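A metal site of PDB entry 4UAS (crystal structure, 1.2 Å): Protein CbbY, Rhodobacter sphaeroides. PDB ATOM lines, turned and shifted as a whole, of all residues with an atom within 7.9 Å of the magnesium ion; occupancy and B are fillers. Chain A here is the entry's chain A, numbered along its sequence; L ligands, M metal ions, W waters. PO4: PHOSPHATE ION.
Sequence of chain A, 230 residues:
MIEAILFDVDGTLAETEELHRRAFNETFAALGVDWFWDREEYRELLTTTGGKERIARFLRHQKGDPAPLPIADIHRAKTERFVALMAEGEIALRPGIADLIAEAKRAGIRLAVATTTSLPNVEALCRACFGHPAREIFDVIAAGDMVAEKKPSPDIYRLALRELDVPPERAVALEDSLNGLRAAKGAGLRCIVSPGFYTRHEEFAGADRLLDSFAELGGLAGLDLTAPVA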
ATOM      1  N   PHE A   7      16.811   0.544  14.003  1.00  0.00           N
ATOM      2  CA  PHE A   7      16.382  -0.532  13.135  1.00  0.00           C
ATOM      3  C   PHE A   7      14.891  -0.709  13.081  1.00  0.00           C
ATOM      4  O   PHE A   7      14.226  -0.886  14.077  1.00  0.00           O
ATOM      5  CB  PHE A   7      16.935  -1.873  13.605  1.00  0.00           C
ATOM      6  CG  PHE A   7      18.435  -1.981  13.563  1.00  0.00           C
ATOM      7  CD1 PHE A   7      19.073  -2.590  12.482  1.00  0.00           C
ATOM      8  CD2 PHE A   7      19.225  -1.526  14.603  1.00  0.00           C
ATOM      9  CE1 PHE A   7      20.474  -2.752  12.484  1.00  0.00           C
ATOM     10  CE2 PHE A   7      20.588  -1.634  14.551  1.00  0.00           C
ATOM     11  CZ  PHE A   7      21.207  -2.268  13.519  1.00  0.00           C
ATOM     12  N   ASP A   8      14.342  -0.701  11.845  1.00  0.00           N
ATOM     13  CA  ASP A   8      13.087  -1.312  11.562  1.00  0.00           C
ATOM     14  C   ASP A   8      13.169  -2.809  11.896  1.00  0.00           C
ATOM     15  O   ASP A   8      14.252  -3.374  11.930  1.00  0.00           O
ATOM     16  CB  ASP A   8      12.798  -1.100  10.088  1.00  0.00           C
ATOM     17  CG  ASP A   8      11.496  -1.617   9.630  1.00  0.00           C
ATOM     18  OD1 ASP A   8      10.470  -1.322  10.302  1.00  0.00           O
ATOM     19  OD2 ASP A   8      11.432  -2.456   8.705  1.00  0.00           O
ATOM     20  N   VAL A   9      12.024  -3.450  12.064  1.00  0.00           N
ATOM     21  CA  VAL A   9      11.981  -4.886  12.320  1.00  0.00           C
ATOM     22  C   VAL A   9      11.575  -5.708  11.093  1.00  0.00           C
ATOM     23  O   VAL A   9      12.380  -6.409  10.506  1.00  0.00           O
ATOM     24  CB  VAL A   9      11.122  -5.235  13.583  1.00  0.00           C
ATOM     25  CG1 VAL A   9      10.999  -6.741  13.763  1.00  0.00           C
ATOM     26  CG2 VAL A   9      11.731  -4.588  14.807  1.00  0.00           C
ATOM     27  N   ASP A  10      10.313  -5.613  10.716  1.00  0.00           N
ATOM     28  CA  ASP A  10       9.774  -6.467   9.653  1.00  0.00           C
ATOM     29  C   ASP A  10      10.366  -6.106   8.304  1.00  0.00           C
ATOM     30  O   ASP A  10      10.191  -5.020   7.809  1.00  0.00           O
ATOM     31  CB  ASP A  10       8.257  -6.371   9.601  1.00  0.00           C
ATOM     32  CG  ASP A  10       7.587  -6.857  10.856  1.00  0.00           C
ATOM     33  OD1 ASP A  10       7.901  -7.980  11.301  1.00  0.00           O
ATOM     34  OD2 ASP A  10       6.764  -6.070  11.414  1.00  0.00           O
ATOM     35  N   GLY A  11      11.036  -7.102   7.708  1.00  0.00           N
ATOM     36  CA  GLY A  11      11.687  -6.907   6.433  1.00  0.00           C
ATOM     37  C   GLY A  11      13.054  -6.301   6.518  1.00  0.00           C
ATOM     38  O   GLY A  11      13.707  -6.210   5.500  1.00  0.00           O
ATOM     39  N   THR A  12      13.514  -5.929   7.714  1.00  0.00           N
ATOM     40  CA  THR A  12      14.807  -5.283   7.949  1.00  0.00           C
ATOM     41  C   THR A  12      15.696  -6.202   8.750  1.00  0.00           C
ATOM     42  O   THR A  12      16.760  -6.651   8.263  1.00  0.00           O
ATOM     43  CB  THR A  12      14.622  -3.872   8.492  1.00  0.00           C
ATOM     44  OG1 THR A  12      13.966  -3.048   7.564  1.00  0.00           O
ATOM     45  CG2 THR A  12      15.942  -3.242   8.856  1.00  0.00           C
ATOM     46  N   LEU A  13      15.344  -6.452  10.001  1.00  0.00           N
ATOM     47  CA  LEU A  13      16.095  -7.430  10.763  1.00  0.00           C
ATOM     48  C   LEU A  13      15.983  -8.830  10.141  1.00  0.00           C
ATOM     49  O   LEU A  13      16.921  -9.598  10.199  1.00  0.00           O
ATOM     50  CB  LEU A  13      15.647  -7.502  12.236  1.00  0.00           C
ATOM     51  CG  LEU A  13      15.911  -6.237  13.070  1.00  0.00           C
ATOM     52  CD1 LEU A  13      15.352  -6.402  14.450  1.00  0.00           C
ATOM     53  CD2 LEU A  13      17.352  -5.845  13.126  1.00  0.00           C
ATOM     54  N   ALA A  14      14.796  -9.200   9.646  1.00  0.00           N
ATOM     55  CA  ALA A  14      14.474 -10.518   9.176  1.00  0.00           C
ATOM     56  C   ALA A  14      13.331 -10.390   8.207  1.00  0.00           C
ATOM     57  O   ALA A  14      12.514  -9.496   8.336  1.00  0.00           O
ATOM     58  CB  ALA A  14      14.173 -11.462  10.304  1.00  0.00           C
ATOM     59  N   THR A  16       9.998 -11.433   7.748  1.00  0.00           N
ATOM     60  CA  THR A  16       8.954 -11.928   8.651  1.00  0.00           C
ATOM     61  C   THR A  16       7.593 -11.948   8.032  1.00  0.00           C
ATOM     62  O   THR A  16       6.667 -12.543   8.592  1.00  0.00           O
ATOM     63  CB  THR A  16       8.841 -11.011   9.884  1.00  0.00           C
ATOM     64  OG1 THR A  16       8.596  -9.704   9.402  1.00  0.00           O
ATOM     65  CG2 THR A  16      10.112 -11.043  10.738  1.00  0.00           C
ATOM     66  N   GLU A  17       7.326 -11.199   6.929  1.00  0.00           N
ATOM     67  CA  GLU A  17       5.949 -10.960   6.521  1.00  0.00           C
ATOM     68  C   GLU A  17       5.268 -12.187   6.033  1.00  0.00           C
ATOM     69  O   GLU A  17       4.020 -12.286   6.249  1.00  0.00           O
ATOM     70  CB  GLU A  17       5.789  -9.840   5.552  1.00  0.00           C
ATOM     71  CG  GLU A  17       5.992  -8.474   6.244  1.00  0.00           C
ATOM     72  CD  GLU A  17       4.950  -8.056   7.253  1.00  0.00           C
ATOM     73  OE1 GLU A  17       3.947  -8.748   7.557  1.00  0.00           O
ATOM     74  OE2 GLU A  17       5.141  -6.973   7.852  1.00  0.00           O
ATOM     75  N   THR A  49       0.281  -0.059   8.190  1.00  0.00           N
ATOM     76  CA  THR A  49       1.136  -0.669   9.169  1.00  0.00           C
ATOM     77  C   THR A  49       0.337  -0.908  10.456  1.00  0.00           C
ATOM     78  O   THR A  49      -0.629  -0.194  10.781  1.00  0.00           O
ATOM     79  CB  THR A  49       2.348   0.190   9.413  1.00  0.00           C
ATOM     80  OG1 THR A  49       1.998   1.363  10.115  1.00  0.00           O
ATOM     81  CG2 THR A  49       3.187   0.471   8.154  1.00  0.00           C
ATOM     82  N   ALA A 114      12.710   0.632  16.095  1.00  0.00           N
ATOM     83  CA  ALA A 114      11.619   1.551  15.840  1.00  0.00           C
ATOM     84  C   ALA A 114      10.672   0.848  14.871  1.00  0.00           C
ATOM     85  O   ALA A 114      11.021   0.740  13.677  1.00  0.00           O
ATOM     86  CB  ALA A 114      12.118   2.861  15.297  1.00  0.00           C
ATOM     87  N   THR A 115       9.554   0.320  15.362  1.00  0.00           N
ATOM     88  CA  THR A 115       8.721  -0.606  14.634  1.00  0.00           C
ATOM     89  C   THR A 115       7.258  -0.351  14.867  1.00  0.00           C
ATOM     90  O   THR A 115       6.855   0.083  15.940  1.00  0.00           O
ATOM     91  CB  THR A 115       9.085  -2.081  15.033  1.00  0.00           C
ATOM     92  OG1 THR A 115       8.296  -2.998  14.248  1.00  0.00           O
ATOM     93  CG2 THR A 115       8.881  -2.329  16.428  1.00  0.00           C
ATOM     94  N   THR A 116       6.460  -0.729  13.879  1.00  0.00           N
ATOM     95  CA  THR A 116       5.019  -0.808  13.972  1.00  0.00           C
ATOM     96  C   THR A 116       4.516  -2.110  14.511  1.00  0.00           C
ATOM     97  O   THR A 116       3.293  -2.177  14.832  1.00  0.00           O
ATOM     98  CB  THR A 116       4.339  -0.553  12.599  1.00  0.00           C
ATOM     99  OG1 THR A 116       4.589  -1.649  11.716  1.00  0.00           O
ATOM    100  CG2 THR A 116       4.823   0.750  11.972  1.00  0.00           C
ATOM    101  N   LYS A 151       3.882   4.414  11.393  1.00  0.00           N
ATOM    102  CA  LYS A 151       4.567   4.709  10.119  1.00  0.00           C
ATOM    103  C   LYS A 151       3.507   4.711   9.007  1.00  0.00           C
ATOM    104  O   LYS A 151       2.661   3.810   8.948  1.00  0.00           O
ATOM    105  CB  LYS A 151       5.679   3.699   9.828  1.00  0.00           C
ATOM    106  CG  LYS A 151       6.764   3.628  10.914  1.00  0.00           C
ATOM    107  CD  LYS A 151       7.895   2.672  10.502  1.00  0.00           C
ATOM    108  CE  LYS A 151       8.755   2.238  11.640  1.00  0.00           C
ATOM    109  NZ  LYS A 151       9.696   1.157  11.233  1.00  0.00           N
ATOM    110  N   TYR A 157       9.892   6.967  15.529  1.00  0.00           N
ATOM    111  CA  TYR A 157      11.283   7.379  15.492  1.00  0.00           C
ATOM    112  C   TYR A 157      11.586   8.503  16.425  1.00  0.00           C
ATOM    113  O   TYR A 157      12.631   8.539  17.079  1.00  0.00           O
ATOM    114  CB  TYR A 157      11.726   7.705  14.062  1.00  0.00           C
ATOM    115  CG  TYR A 157      12.042   6.508  13.174  1.00  0.00           C
ATOM    116  CD1 TYR A 157      11.228   6.090  12.164  1.00  0.00           C
ATOM    117  CD2 TYR A 157      13.218   5.812  13.382  1.00  0.00           C
ATOM    118  CE1 TYR A 157      11.568   4.998  11.354  1.00  0.00           C
ATOM    119  CE2 TYR A 157      13.574   4.741  12.604  1.00  0.00           C
ATOM    120  CZ  TYR A 157      12.746   4.309  11.604  1.00  0.00           C
ATOM    121  OH  TYR A 157      13.145   3.270  10.825  1.00  0.00           O
ATOM    122  N   LEU A 174      17.793   2.075   9.482  1.00  0.00           N
ATOM    123  CA  LEU A 174      17.743   1.000   8.459  1.00  0.00           C
ATOM    124  C   LEU A 174      16.307   0.590   8.298  1.00  0.00           C
ATOM    125  O   LEU A 174      15.587   0.314   9.263  1.00  0.00           O
ATOM    126  CB  LEU A 174      18.553  -0.206   8.839  1.00  0.00           C
ATOM    127  CG  LEU A 174      20.036  -0.153   8.549  1.00  0.00           C
ATOM    128  CD1 LEU A 174      20.728   0.931   9.221  1.00  0.00           C
ATOM    129  CD2 LEU A 174      20.661  -1.483   8.820  1.00  0.00           C
ATOM    130  N   GLU A 175      15.843   0.580   7.034  1.00  0.00           N
ATOM    131  CA  GLU A 175      14.444   0.340   6.668  1.00  0.00           C
ATOM    132  C   GLU A 175      14.373  -0.507   5.420  1.00  0.00           C
ATOM    133  O   GLU A 175      15.325  -0.708   4.691  1.00  0.00           O
ATOM    134  CB  GLU A 175      13.734   1.686   6.392  1.00  0.00           C
ATOM    135  CG  GLU A 175      13.179   2.311   7.667  1.00  0.00           C
ATOM    136  CD  GLU A 175      11.945   1.631   8.186  1.00  0.00           C
ATOM    137  OE1 GLU A 175      11.477   0.665   7.507  1.00  0.00           O
ATOM    138  OE2 GLU A 175      11.457   2.082   9.253  1.00  0.00           O
ATOM    139  N   ASP A 176      13.142  -1.042   5.151  1.00  0.00           N
ATOM    140  CA  ASP A 176      12.865  -1.839   4.003  1.00  0.00           C
ATOM    141  C   ASP A 176      11.707  -1.360   3.176  1.00  0.00           C
ATOM    142  O   ASP A 176      11.453  -1.946   2.110  1.00  0.00           O
ATOM    143  CB  ASP A 176      12.602  -3.319   4.353  1.00  0.00           C
ATOM    144  CG  ASP A 176      11.228  -3.468   4.991  1.00  0.00           C
ATOM    145  OD1 ASP A 176      11.011  -2.752   5.980  1.00  0.00           O
ATOM    146  OD2 ASP A 176      10.386  -4.280   4.546  1.00  0.00           O
ATOM    147  N   SER A 177      10.921  -0.382   3.609  1.00  0.00           N
ATOM    148  CA  SER A 177       9.687   0.004   2.989  1.00  0.00           C
ATOM    149  C   SER A 177       9.583   1.482   2.862  1.00  0.00           C
ATOM    150  O   SER A 177      10.240   2.260   3.581  1.00  0.00           O
ATOM    151  CB  SER A 177       8.498  -0.504   3.777  1.00  0.00           C
ATOM    152  OG  SER A 177       8.304   0.251   4.970  1.00  0.00           O
ATOM    153  N   LEU A 178       8.711   1.947   1.982  1.00  0.00           N
ATOM    154  CA  LEU A 178       8.475   3.358   1.763  1.00  0.00           C
ATOM    155  C   LEU A 178       7.837   4.017   2.989  1.00  0.00           C
ATOM    156  O   LEU A 178       8.259   5.106   3.364  1.00  0.00           O
ATOM    157  CB  LEU A 178       7.667   3.591   0.514  1.00  0.00           C
ATOM    158  CG  LEU A 178       7.325   5.030   0.174  1.00  0.00           C
ATOM    159  CD1 LEU A 178       8.602   5.905   0.070  1.00  0.00           C
ATOM    160  CD2 LEU A 178       6.517   5.110  -1.100  1.00  0.00           C
ATOM    161  N   ASN A 179       6.881   3.374   3.612  1.00  0.00           N
ATOM    162  CA  ASN A 179       6.344   3.925   4.831  1.00  0.00           C
ATOM    163  C   ASN A 179       7.427   4.142   5.874  1.00  0.00           C
ATOM    164  O   ASN A 179       7.413   5.130   6.624  1.00  0.00           O
ATOM    165  CB  ASN A 179       5.257   3.066   5.404  1.00  0.00           C
ATOM    166  CG  ASN A 179       3.909   3.149   4.730  1.00  0.00           C
ATOM    167  OD1 ASN A 179       3.134   2.088   4.718  1.00  0.00           O
ATOM    168  ND2 ASN A 179       3.561   4.244   4.259  1.00  0.00           N
ATOM    169  N   GLY A 180       8.331   3.198   5.947  1.00  0.00           N
ATOM    170  CA  GLY A 180       9.451   3.293   6.910  1.00  0.00           C
ATOM    171  C   GLY A 180      10.438   4.434   6.585  1.00  0.00           C
ATOM    172  O   GLY A 180      10.827   5.185   7.466  1.00  0.00           O
ATOM    173  N   LEU A 181      10.794   4.522   5.313  1.00  0.00           N
ATOM    174  CA  LEU A 181      11.649   5.605   4.836  1.00  0.00           C
ATOM    175  C   LEU A 181      11.055   6.933   5.173  1.00  0.00           C
ATOM    176  O   LEU A 181      11.709   7.851   5.664  1.00  0.00           O
ATOM    177  CB  LEU A 181      11.893   5.437   3.339  1.00  0.00           C
ATOM    178  CG  LEU A 181      12.605   6.600   2.653  1.00  0.00           C
ATOM    179  CD1 LEU A 181      13.994   6.849   3.163  1.00  0.00           C
ATOM    180  CD2 LEU A 181      12.647   6.349   1.164  1.00  0.00           C
ATOM    181  N   SER A 194      17.027  -1.317   2.272  1.00  0.00           N
ATOM    182  CA  SER A 194      17.205  -2.545   1.469  1.00  0.00           C
ATOM    183  C   SER A 194      15.868  -3.227   1.394  1.00  0.00           C
ATOM    184  O   SER A 194      15.342  -3.700   2.402  1.00  0.00           O
ATOM    185  CB  SER A 194      18.212  -3.493   2.036  1.00  0.00           C
ATOM    186  OG  SER A 194      18.385  -4.611   1.132  1.00  0.00           O
ATOM    187  N   THR A 199       8.242  -5.287  -0.835  1.00  0.00           N
ATOM    188  CA  THR A 199       8.510  -3.857  -1.025  1.00  0.00           C
ATOM    189  C   THR A 199       9.356  -3.516  -2.236  1.00  0.00           C
ATOM    190  O   THR A 199       9.589  -2.365  -2.483  1.00  0.00           O
ATOM    191  CB  THR A 199       9.080  -3.229   0.227  1.00  0.00           C
ATOM    192  OG1 THR A 199      10.349  -3.862   0.478  1.00  0.00           O
ATOM    193  CG2 THR A 199       8.130  -3.341   1.397  1.00  0.00           C
HETATM  194  P   PO4 L   1       7.913  -2.718  10.818  1.00  0.00           P
HETATM  195  O1  PO4 L   1       7.514  -1.226  11.175  1.00  0.00           O
HETATM  196  O2  PO4 L   1       6.583  -3.577  10.878  1.00  0.00           O
HETATM  197  O3  PO4 L   1       8.901  -3.400  11.754  1.00  0.00           O
HETATM  198  O4  PO4 L   1       8.410  -2.827   9.338  1.00  0.00           O
HETATM  199 MG    MG M   1       9.659  -2.908   7.649  1.00  0.00          MG
HETATM  200  O   HOH W   1       8.256  -3.411   6.328  1.00  0.00           O
HETATM  201  O   HOH W   2       9.279  -0.754   7.328  1.00  0.00           O
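Three residues have an atom within 4 Å of the magnesium ion: Asp 8, Asp 10 and Asp 176. The nearest printed residue that does not touch the magnesium ion is Glu 175 (4.01 Å).
The magnesium ion is bound by water W1 (2.0 Å), O4 of the ligand (2.1 Å), OD2 of Asp 8 (2.1 Å), OD1 of Asp 176 (2.2 Å), O of Asp 10 (2.2 Å) and water W2 (2.2 Å). The magnesium ion has six donor atoms within binding distance.
Water W2 lies within hydrogen-bond range of OE1 of Glu 175, OG of Ser 177 and OD1 of Asp 8.
The side-chain hydroxyl (OG1) of Thr 12 sits close to the side-chain carboxylate (OD2) of Asp 8 (2.8 Å). OD1 of Asp 8 is in salt-bridge range of NZ of Lys 151 (2.8 Å). The backbone NH (N) of Asp 8 is in hydrogen-bond range of the backbone carbonyl oxygen (O) of Leu 174, at 3.0 Å. The side-chain hydroxyl of Thr 12 lies within hydrogen-bond range of the backbone NH of Asp 176, at 3.2 Å. O of Asp 176 sits at hydrogen-bond distance from OG1 of Thr 199 (2.7 Å). The side-chain carboxylate (OD1) of Asp 10 lies within hydrogen-bond range of the side-chain hydroxyl (OG1) of Thr 16, 2.7 Å away.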
